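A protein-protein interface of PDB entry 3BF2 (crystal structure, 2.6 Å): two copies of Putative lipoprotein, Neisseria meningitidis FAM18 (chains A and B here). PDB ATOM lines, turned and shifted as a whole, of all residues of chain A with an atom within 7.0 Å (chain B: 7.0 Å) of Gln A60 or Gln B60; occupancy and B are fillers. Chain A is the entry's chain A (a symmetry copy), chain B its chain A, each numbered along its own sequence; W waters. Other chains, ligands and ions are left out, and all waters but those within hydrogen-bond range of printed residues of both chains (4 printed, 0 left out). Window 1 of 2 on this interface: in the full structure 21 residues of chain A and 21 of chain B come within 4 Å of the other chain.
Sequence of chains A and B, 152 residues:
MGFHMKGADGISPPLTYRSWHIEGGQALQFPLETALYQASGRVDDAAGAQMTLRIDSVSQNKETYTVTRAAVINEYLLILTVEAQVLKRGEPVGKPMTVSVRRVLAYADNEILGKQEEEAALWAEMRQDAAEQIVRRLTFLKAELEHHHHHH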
ATOM      1  N   ALA A  27      19.792  25.173  14.702  1.00  0.00           N
ATOM      2  CA  ALA A  27      19.146  24.294  15.670  1.00  0.00           C
ATOM      3  C   ALA A  27      17.634  24.475  15.718  1.00  0.00           C
ATOM      4  O   ALA A  27      16.907  23.571  16.129  1.00  0.00           O
ATOM      5  CB  ALA A  27      19.739  24.508  17.046  1.00  0.00           C
ATOM      6  N   VAL A  58      20.754  33.519  19.123  1.00  0.00           N
ATOM      7  CA  VAL A  58      20.160  32.416  19.865  1.00  0.00           C
ATOM      8  C   VAL A  58      20.984  32.304  21.128  1.00  0.00           C
ATOM      9  O   VAL A  58      22.201  32.213  21.082  1.00  0.00           O
ATOM     10  CB  VAL A  58      20.214  31.093  19.088  1.00  0.00           C
ATOM     11  CG1 VAL A  58      19.622  29.975  19.942  1.00  0.00           C
ATOM     12  CG2 VAL A  58      19.424  31.226  17.797  1.00  0.00           C
ATOM     13  N   SER A  59      20.316  32.348  22.265  1.00  0.00           N
ATOM     14  CA  SER A  59      21.007  32.291  23.535  1.00  0.00           C
ATOM     15  C   SER A  59      20.459  31.207  24.450  1.00  0.00           C
ATOM     16  O   SER A  59      19.244  31.082  24.608  1.00  0.00           O
ATOM     17  CB  SER A  59      20.908  33.660  24.212  1.00  0.00           C
ATOM     18  OG  SER A  59      21.163  33.586  25.606  1.00  0.00           O
ATOM     19  N   GLN A  60      21.371  30.430  25.034  1.00  0.00           N
ATOM     20  CA  GLN A  60      21.024  29.367  25.978  1.00  0.00           C
ATOM     21  C   GLN A  60      21.786  29.630  27.263  1.00  0.00           C
ATOM     22  O   GLN A  60      23.002  29.438  27.333  1.00  0.00           O
ATOM     23  CB  GLN A  60      21.399  27.991  25.440  1.00  0.00           C
ATOM     24  CG  GLN A  60      20.633  27.617  24.190  1.00  0.00           C
ATOM     25  CD  GLN A  60      20.903  26.198  23.743  1.00  0.00           C
ATOM     26  OE1 GLN A  60      20.486  25.790  22.657  1.00  0.00           O
ATOM     27  NE2 GLN A  60      21.589  25.429  24.586  1.00  0.00           N
ATOM     28  N   ASN A  61      21.064  30.082  28.283  1.00  0.00           N
ATOM     29  CA  ASN A  61      21.672  30.396  29.561  1.00  0.00           C
ATOM     30  C   ASN A  61      21.185  29.447  30.662  1.00  0.00           C
ATOM     31  O   ASN A  61      19.982  29.258  30.856  1.00  0.00           O
ATOM     32  CB  ASN A  61      21.368  31.865  29.893  1.00  0.00           C
ATOM     33  CG  ASN A  61      21.980  32.318  31.211  1.00  0.00           C
ATOM     34  OD1 ASN A  61      22.914  31.698  31.729  1.00  0.00           O
ATOM     35  ND2 ASN A  61      21.460  33.414  31.755  1.00  0.00           N
ATOM     36  N   LYS A  62      22.131  28.824  31.357  1.00  0.00           N
ATOM     37  CA  LYS A  62      21.815  27.899  32.444  1.00  0.00           C
ATOM     38  C   LYS A  62      22.290  28.576  33.726  1.00  0.00           C
ATOM     39  O   LYS A  62      23.482  28.844  33.900  1.00  0.00           O
ATOM     40  CB  LYS A  62      22.544  26.569  32.254  1.00  0.00           C
ATOM     41  CG  LYS A  62      22.158  25.509  33.283  1.00  0.00           C
ATOM     42  CD  LYS A  62      22.886  24.201  33.042  1.00  0.00           C
ATOM     43  CE  LYS A  62      24.379  24.349  33.308  1.00  0.00           C
ATOM     44  NZ  LYS A  62      25.182  23.284  32.632  1.00  0.00           N
ATOM     45  N   LEU A  78      16.728  27.483  33.219  1.00  0.00           N
ATOM     46  CA  LEU A  78      17.214  27.499  31.843  1.00  0.00           C
ATOM     47  C   LEU A  78      16.421  28.543  31.045  1.00  0.00           C
ATOM     48  O   LEU A  78      15.185  28.579  31.112  1.00  0.00           O
ATOM     49  CB  LEU A  78      17.057  26.113  31.189  1.00  0.00           C
ATOM     50  CG  LEU A  78      17.672  24.871  31.868  1.00  0.00           C
ATOM     51  CD1 LEU A  78      17.389  23.660  31.033  1.00  0.00           C
ATOM     52  CD2 LEU A  78      19.176  25.009  32.026  1.00  0.00           C
ATOM     53  N   ILE A  79      17.127  29.401  30.308  1.00  0.00           N
ATOM     54  CA  ILE A  79      16.479  30.419  29.488  1.00  0.00           C
ATOM     55  C   ILE A  79      16.949  30.370  28.032  1.00  0.00           C
ATOM     56  O   ILE A  79      18.143  30.497  27.732  1.00  0.00           O
ATOM     57  CB  ILE A  79      16.739  31.854  30.024  1.00  0.00           C
ATOM     58  CG1 ILE A  79      16.147  32.033  31.431  1.00  0.00           C
ATOM     59  CG2 ILE A  79      16.102  32.879  29.080  1.00  0.00           C
ATOM     60  CD1 ILE A  79      17.109  31.674  32.556  1.00  0.00           C
ATOM     61  N   LEU A  80      16.004  30.176  27.119  1.00  0.00           N
ATOM     62  CA  LEU A  80      16.316  30.134  25.691  1.00  0.00           C
ATOM     63  C   LEU A  80      15.802  31.453  25.114  1.00  0.00           C
ATOM     64  O   LEU A  80      14.627  31.808  25.267  1.00  0.00           O
ATOM     65  CB  LEU A  80      15.616  28.938  25.038  1.00  0.00           C
ATOM     66  CG  LEU A  80      15.925  28.401  23.623  1.00  0.00           C
ATOM     67  CD1 LEU A  80      14.897  28.917  22.660  1.00  0.00           C
ATOM     68  CD2 LEU A  80      17.336  28.777  23.181  1.00  0.00           C
ATOM     69  N   THR A  81      16.696  32.203  24.486  1.00  0.00           N
ATOM     70  CA  THR A  81      16.311  33.470  23.902  1.00  0.00           C
ATOM     71  C   THR A  81      16.651  33.480  22.426  1.00  0.00           C
ATOM     72  O   THR A  81      17.765  33.124  22.025  1.00  0.00           O
ATOM     73  CB  THR A  81      17.032  34.635  24.592  1.00  0.00           C
ATOM     74  OG1 THR A  81      16.698  34.628  25.985  1.00  0.00           O
ATOM     75  CG2 THR A  81      16.617  35.972  23.972  1.00  0.00           C
ATOM     76  N   GLU A 119      19.077  17.338  30.209  1.00  0.00           N
ATOM     77  CA  GLU A 119      19.157  18.764  29.927  1.00  0.00           C
ATOM     78  C   GLU A 119      18.964  18.971  28.432  1.00  0.00           C
ATOM     79  O   GLU A 119      18.292  19.906  28.004  1.00  0.00           O
ATOM     80  CB  GLU A 119      20.513  19.345  30.345  1.00  0.00           C
ATOM     81  CG  GLU A 119      20.516  20.874  30.391  1.00  0.00           C
ATOM     82  CD  GLU A 119      21.898  21.503  30.274  1.00  0.00           C
ATOM     83  OE1 GLU A 119      22.805  21.144  31.056  1.00  0.00           O
ATOM     84  OE2 GLU A 119      22.080  22.369  29.393  1.00  0.00           O
ATOM     85  N   TRP A 123      16.222  21.369  26.465  1.00  0.00           N
ATOM     86  CA  TRP A 123      16.567  22.377  25.466  1.00  0.00           C
ATOM     87  C   TRP A 123      15.815  22.072  24.177  1.00  0.00           C
ATOM     88  O   TRP A 123      15.399  22.975  23.446  1.00  0.00           O
ATOM     89  CB  TRP A 123      18.067  22.390  25.176  1.00  0.00           C
ATOM     90  CG  TRP A 123      18.910  23.053  26.228  1.00  0.00           C
ATOM     91  CD1 TRP A 123      19.954  22.492  26.898  1.00  0.00           C
ATOM     92  CD2 TRP A 123      18.806  24.409  26.712  1.00  0.00           C
ATOM     93  NE1 TRP A 123      20.508  23.406  27.763  1.00  0.00           N
ATOM     94  CE2 TRP A 123      19.827  24.589  27.663  1.00  0.00           C
ATOM     95  CE3 TRP A 123      17.958  25.481  26.425  1.00  0.00           C
ATOM     96  CZ2 TRP A 123      20.014  25.798  28.342  1.00  0.00           C
ATOM     97  CZ3 TRP A 123      18.144  26.680  27.101  1.00  0.00           C
ATOM     98  CH2 TRP A 123      19.170  26.828  28.046  1.00  0.00           C
ATOM     99  N   ARG A 127      13.256  24.507  22.385  1.00  0.00           N
ATOM    100  CA  ARG A 127      13.438  24.969  21.036  1.00  0.00           C
ATOM    101  C   ARG A 127      12.149  24.816  20.260  1.00  0.00           C
ATOM    102  O   ARG A 127      11.828  25.645  19.416  1.00  0.00           O
ATOM    103  CB  ARG A 127      14.579  24.216  20.363  1.00  0.00           C
ATOM    104  CG  ARG A 127      15.960  24.697  20.814  1.00  0.00           C
ATOM    105  CD  ARG A 127      17.061  24.126  19.929  1.00  0.00           C
ATOM    106  NE  ARG A 127      17.390  22.748  20.277  1.00  0.00           N
ATOM    107  CZ  ARG A 127      18.353  22.403  21.125  1.00  0.00           C
ATOM    108  NH1 ARG A 127      19.100  23.332  21.716  1.00  0.00           N
ATOM    109  NH2 ARG A 127      18.560  21.127  21.400  1.00  0.00           N
ATOM    110  N   ALA B  27      28.152  19.947  31.843  1.00  0.00           N
ATOM    111  CA  ALA B  27      28.848  19.882  30.563  1.00  0.00           C
ATOM    112  C   ALA B  27      30.334  20.199  30.679  1.00  0.00           C
ATOM    113  O   ALA B  27      31.130  19.791  29.835  1.00  0.00           O
ATOM    114  CB  ALA B  27      28.195  20.815  29.566  1.00  0.00           C
ATOM    115  N   VAL B  58      26.262  29.147  33.225  1.00  0.00           N
ATOM    116  CA  VAL B  58      26.935  28.764  31.991  1.00  0.00           C
ATOM    117  C   VAL B  58      26.086  29.348  30.884  1.00  0.00           C
ATOM    118  O   VAL B  58      24.885  29.131  30.829  1.00  0.00           O
ATOM    119  CB  VAL B  58      27.032  27.241  31.827  1.00  0.00           C
ATOM    120  CG1 VAL B  58      27.700  26.912  30.495  1.00  0.00           C
ATOM    121  CG2 VAL B  58      27.845  26.654  32.968  1.00  0.00           C
ATOM    122  N   SER B  59      26.711  30.122  30.018  1.00  0.00           N
ATOM    123  CA  SER B  59      25.989  30.766  28.942  1.00  0.00           C
ATOM    124  C   SER B  59      26.609  30.497  27.580  1.00  0.00           C
ATOM    125  O   SER B  59      27.824  30.607  27.417  1.00  0.00           O
ATOM    126  CB  SER B  59      25.936  32.272  29.216  1.00  0.00           C
ATOM    127  OG  SER B  59      25.645  33.017  28.044  1.00  0.00           O
ATOM    128  N   GLN B  60      25.756  30.137  26.620  1.00  0.00           N
ATOM    129  CA  GLN B  60      26.173  29.884  25.240  1.00  0.00           C
ATOM    130  C   GLN B  60      25.350  30.785  24.340  1.00  0.00           C
ATOM    131  O   GLN B  60      24.156  30.558  24.132  1.00  0.00           O
ATOM    132  CB  GLN B  60      25.947  28.430  24.842  1.00  0.00           C
ATOM    133  CG  GLN B  60      26.785  27.460  25.648  1.00  0.00           C
ATOM    134  CD  GLN B  60      26.665  26.036  25.154  1.00  0.00           C
ATOM    135  OE1 GLN B  60      27.153  25.104  25.798  1.00  0.00           O
ATOM    136  NE2 GLN B  60      26.029  25.858  23.999  1.00  0.00           N
ATOM    137  N   ASN B  61      25.993  31.821  23.813  1.00  0.00           N
ATOM    138  CA  ASN B  61      25.317  32.774  22.954  1.00  0.00           C
ATOM    139  C   ASN B  61      25.858  32.717  21.520  1.00  0.00           C
ATOM    140  O   ASN B  61      27.067  32.796  21.289  1.00  0.00           O
ATOM    141  CB  ASN B  61      25.470  34.173  23.570  1.00  0.00           C
ATOM    142  CG  ASN B  61      24.776  35.260  22.761  1.00  0.00           C
ATOM    143  OD1 ASN B  61      23.889  34.985  21.948  1.00  0.00           O
ATOM    144  ND2 ASN B  61      25.172  36.508  22.993  1.00  0.00           N
ATOM    145  N   LYS B  62      24.954  32.543  20.561  1.00  0.00           N
ATOM    146  CA  LYS B  62      25.322  32.482  19.148  1.00  0.00           C
ATOM    147  C   LYS B  62      24.745  33.739  18.506  1.00  0.00           C
ATOM    148  O   LYS B  62      23.527  33.944  18.488  1.00  0.00           O
ATOM    149  CB  LYS B  62      24.730  31.238  18.487  1.00  0.00           C
ATOM    150  CG  LYS B  62      25.181  31.041  17.042  1.00  0.00           C
ATOM    151  CD  LYS B  62      24.589  29.783  16.435  1.00  0.00           C
ATOM    152  CE  LYS B  62      23.081  29.918  16.262  1.00  0.00           C
ATOM    153  NZ  LYS B  62      22.405  28.589  16.147  1.00  0.00           N
ATOM    154  N   LEU B  78      30.399  33.094  18.438  1.00  0.00           N
ATOM    155  CA  LEU B  78      29.957  32.243  19.538  1.00  0.00           C
ATOM    156  C   LEU B  78      30.672  32.677  20.824  1.00  0.00           C
ATOM    157  O   LEU B  78      31.896  32.862  20.831  1.00  0.00           O
ATOM    158  CB  LEU B  78      30.266  30.762  19.244  1.00  0.00           C
ATOM    159  CG  LEU B  78      29.751  30.116  17.940  1.00  0.00           C
ATOM    160  CD1 LEU B  78      30.173  28.680  17.900  1.00  0.00           C
ATOM    161  CD2 LEU B  78      28.235  30.177  17.848  1.00  0.00           C
ATOM    162  N   ILE B  79      29.911  32.856  21.904  1.00  0.00           N
ATOM    163  CA  ILE B  79      30.485  33.243  23.189  1.00  0.00           C
ATOM    164  C   ILE B  79      30.067  32.293  24.315  1.00  0.00           C
ATOM    165  O   ILE B  79      28.877  32.103  24.594  1.00  0.00           O
ATOM    166  CB  ILE B  79      30.073  34.683  23.604  1.00  0.00           C
ATOM    167  CG1 ILE B  79      30.600  35.719  22.599  1.00  0.00           C
ATOM    168  CG2 ILE B  79      30.638  35.000  24.992  1.00  0.00           C
ATOM    169  CD1 ILE B  79      29.642  36.010  21.452  1.00  0.00           C
ATOM    170  N   LEU B  80      31.055  31.686  24.963  1.00  0.00           N
ATOM    171  CA  LEU B  80      30.793  30.773  26.075  1.00  0.00           C
ATOM    172  C   LEU B  80      31.197  31.532  27.339  1.00  0.00           C
ATOM    173  O   LEU B  80      32.328  32.017  27.465  1.00  0.00           O
ATOM    174  CB  LEU B  80      31.624  29.497  25.911  1.00  0.00           C
ATOM    175  CG  LEU B  80      31.412  28.196  26.718  1.00  0.00           C
ATOM    176  CD1 LEU B  80      32.416  28.134  27.831  1.00  0.00           C
ATOM    177  CD2 LEU B  80      29.986  28.099  27.252  1.00  0.00           C
ATOM    178  N   THR B  81      30.256  31.671  28.261  1.00  0.00           N
ATOM    179  CA  THR B  81      30.537  32.372  29.497  1.00  0.00           C
ATOM    180  C   THR B  81      30.244  31.470  30.678  1.00  0.00           C
ATOM    181  O   THR B  81      29.183  30.841  30.753  1.00  0.00           O
ATOM    182  CB  THR B  81      29.688  33.644  29.612  1.00  0.00           C
ATOM    183  OG1 THR B  81      29.977  34.499  28.500  1.00  0.00           O
ATOM    184  CG2 THR B  81      29.992  34.382  30.919  1.00  0.00           C
ATOM    185  N   GLU B 119      29.121  22.982  14.749  1.00  0.00           N
ATOM    186  CA  GLU B 119      28.915  23.945  15.821  1.00  0.00           C
ATOM    187  C   GLU B 119      29.135  23.240  17.151  1.00  0.00           C
ATOM    188  O   GLU B 119      29.727  23.795  18.072  1.00  0.00           O
ATOM    189  CB  GLU B 119      27.497  24.529  15.789  1.00  0.00           C
ATOM    190  CG  GLU B 119      27.347  25.776  16.660  1.00  0.00           C
ATOM    191  CD  GLU B 119      25.916  26.077  17.084  1.00  0.00           C
ATOM    192  OE1 GLU B 119      25.024  26.170  16.215  1.00  0.00           O
ATOM    193  OE2 GLU B 119      25.681  26.227  18.302  1.00  0.00           O
ATOM    194  N   TRP B 123      31.696  24.246  20.244  1.00  0.00           N
ATOM    195  CA  TRP B 123      31.289  24.423  21.635  1.00  0.00           C
ATOM    196  C   TRP B 123      32.107  23.484  22.513  1.00  0.00           C
ATOM    197  O   TRP B 123      32.458  23.810  23.649  1.00  0.00           O
ATOM    198  CB  TRP B 123      29.804  24.118  21.828  1.00  0.00           C
ATOM    199  CG  TRP B 123      28.869  25.193  21.350  1.00  0.00           C
ATOM    200  CD1 TRP B 123      27.862  25.044  20.446  1.00  0.00           C
ATOM    201  CD2 TRP B 123      28.828  26.573  21.772  1.00  0.00           C
ATOM    202  NE1 TRP B 123      27.197  26.235  20.278  1.00  0.00           N
ATOM    203  CE2 TRP B 123      27.766  27.185  21.083  1.00  0.00           C
ATOM    204  CE3 TRP B 123      29.579  27.339  22.666  1.00  0.00           C
ATOM    205  CZ2 TRP B 123      27.443  28.536  21.251  1.00  0.00           C
ATOM    206  CZ3 TRP B 123      29.259  28.681  22.831  1.00  0.00           C
ATOM    207  CH2 TRP B 123      28.194  29.263  22.128  1.00  0.00           C
ATOM    208  N   ARG B 127      34.477  24.605  25.480  1.00  0.00           N
ATOM    209  CA  ARG B 127      34.295  24.155  26.833  1.00  0.00           C
ATOM    210  C   ARG B 127      35.616  23.693  27.406  1.00  0.00           C
ATOM    211  O   ARG B 127      35.883  23.884  28.588  1.00  0.00           O
ATOM    212  CB  ARG B 127      33.252  23.045  26.890  1.00  0.00           C
ATOM    213  CG  ARG B 127      31.818  23.566  26.771  1.00  0.00           C
ATOM    214  CD  ARG B 127      30.805  22.479  27.107  1.00  0.00           C
ATOM    215  NE  ARG B 127      30.598  21.555  25.998  1.00  0.00           N
ATOM    216  CZ  ARG B 127      29.645  21.693  25.081  1.00  0.00           C
ATOM    217  NH1 ARG B 127      28.796  22.714  25.135  1.00  0.00           N
ATOM    218  NH2 ARG B 127      29.553  20.817  24.095  1.00  0.00           N
HETATM  219  O   HOH W   1      23.346  29.406  21.411  1.00  0.00           O
HETATM  220  O   HOH W   2      27.341  22.761  31.548  1.00  0.00           O
HETATM  221  O   HOH W   3      24.003  26.977  28.859  1.00  0.00           O
HETATM  222  O   HOH W   4      20.341  27.322  16.638  1.00  0.00           O
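The side-chain amide oxygen (OD1) of Asn A61 sits close to the backbone carbonyl oxygen (O) of Val B58.
The backbone NH of Lys A62 is in hydrogen-bond range of the backbone carbonyl oxygen of Val B58, 2.8 Å away.
The backbone NH of Gln A60 sits at hydrogen-bond distance from the backbone carbonyl oxygen of Gln B60, at 2.9 Å.
The backbone carbonyl oxygen of Val A58 lies close to the side-chain amide oxygen of Asn B61, 3.4 Å away.
The backbone NH (N) of Lys B62 is in hydrogen-bond range of the backbone carbonyl oxygen (O) of Val A58.
The side-chain amide oxygen (OE1) of Gln B60 is in hydrogen-bond range of the guanidinium group (NH1) of Arg B127, 3.0 Å away.
The backbone carbonyl oxygen (O) of Asn B61 lies within hydrogen-bond range of the backbone NH (N) of Ile B79.
N of Ser A59 lies within hydrogen-bond range of O of Thr A81 (2.7 Å).
The guanidinium group (NH1) of Arg A127 lies within hydrogen-bond range of the side-chain amide oxygen (OE1) of Gln A60 (3.0 Å).
The backbone NH of Ile A79 lies within hydrogen-bond range of the backbone carbonyl oxygen of Asn A61 (2.9 Å).
The side-chain amino group (NZ) of Lys A62 is in salt-bridge range of the side-chain carboxylate (OE1) of Glu A119 (3.6 Å).
O of Val A58 touches O of Gln B60, at 3.98 Å.
Ser A59 touches Gln B60 (CA to O, 3.6 Å).
Ser A59 touches Asn B61 (CB to OD1, 3.97 Å).
Gln A60 touches Val B58.
Gln A60 touches Ser B59.
CB of Ser B59 touches OD1 of Asn A61, at 3.97 Å.
Of the printed residues of chain B, Val A58 touches Gln B60 (3.98 Å), Asn B61 (3.4 Å) and Lys B62 (2.8 Å).
Printed residues of chain B within 4 Å of Ser A59: Gln B60 and Asn B61.
Of the printed residues of chain B, Gln A60 touches Val B58, Ser B59 and Gln B60.
Printed residues of chain A within 4 Å of Val B58: Gln A60, Asn A61 and Lys A62.
Of the printed residues of chain A, Gln B60 touches Val A58, Ser A59 and Gln A60.
The nearest printed residue of chain B that does not touch Gln A60 is Asn B61 (5.0 Å).
The nearest printed residue of chain B that does not touch Lys A62 is Ala B27 (4.5 Å).
Printed residues of chain A that touch a printed residue of chain B: Val A58, Ser A59, Gln A60, Asn A61 and Lys A62.
Among the printed residues, 11 pairs touch across the chains.
Val A58 touches Gln B60, and with the chains exchanged Gln A60 touches Val B58.
Val A58 touches Lys B62, and with the chains exchanged Lys A62 touches Val B58.
Ser A59 touches Gln B60, and with the chains exchanged Gln A60 touches Ser B59.
Gln A60 touches its own counterpart, Gln B60.
Water W4 lies within hydrogen-bond range of the side-chain amino group (NZ) of Lys B62 and the backbone NH (N) of Ala A27.
Water W2 bridges the side-chain amino group of Lys A62 (2.5 Å) and the backbone NH of Ala B27 (2.9 Å).
Water W3 bridges the backbone carbonyl oxygen of Val B58 (3.0 Å) and the backbone carbonyl oxygen of Gln A60 (3.1 Å).
Water W1 bridges the backbone carbonyl oxygen of Val A58 (3.0 Å) and the backbone carbonyl oxygen of Gln B60 (3.1 Å).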
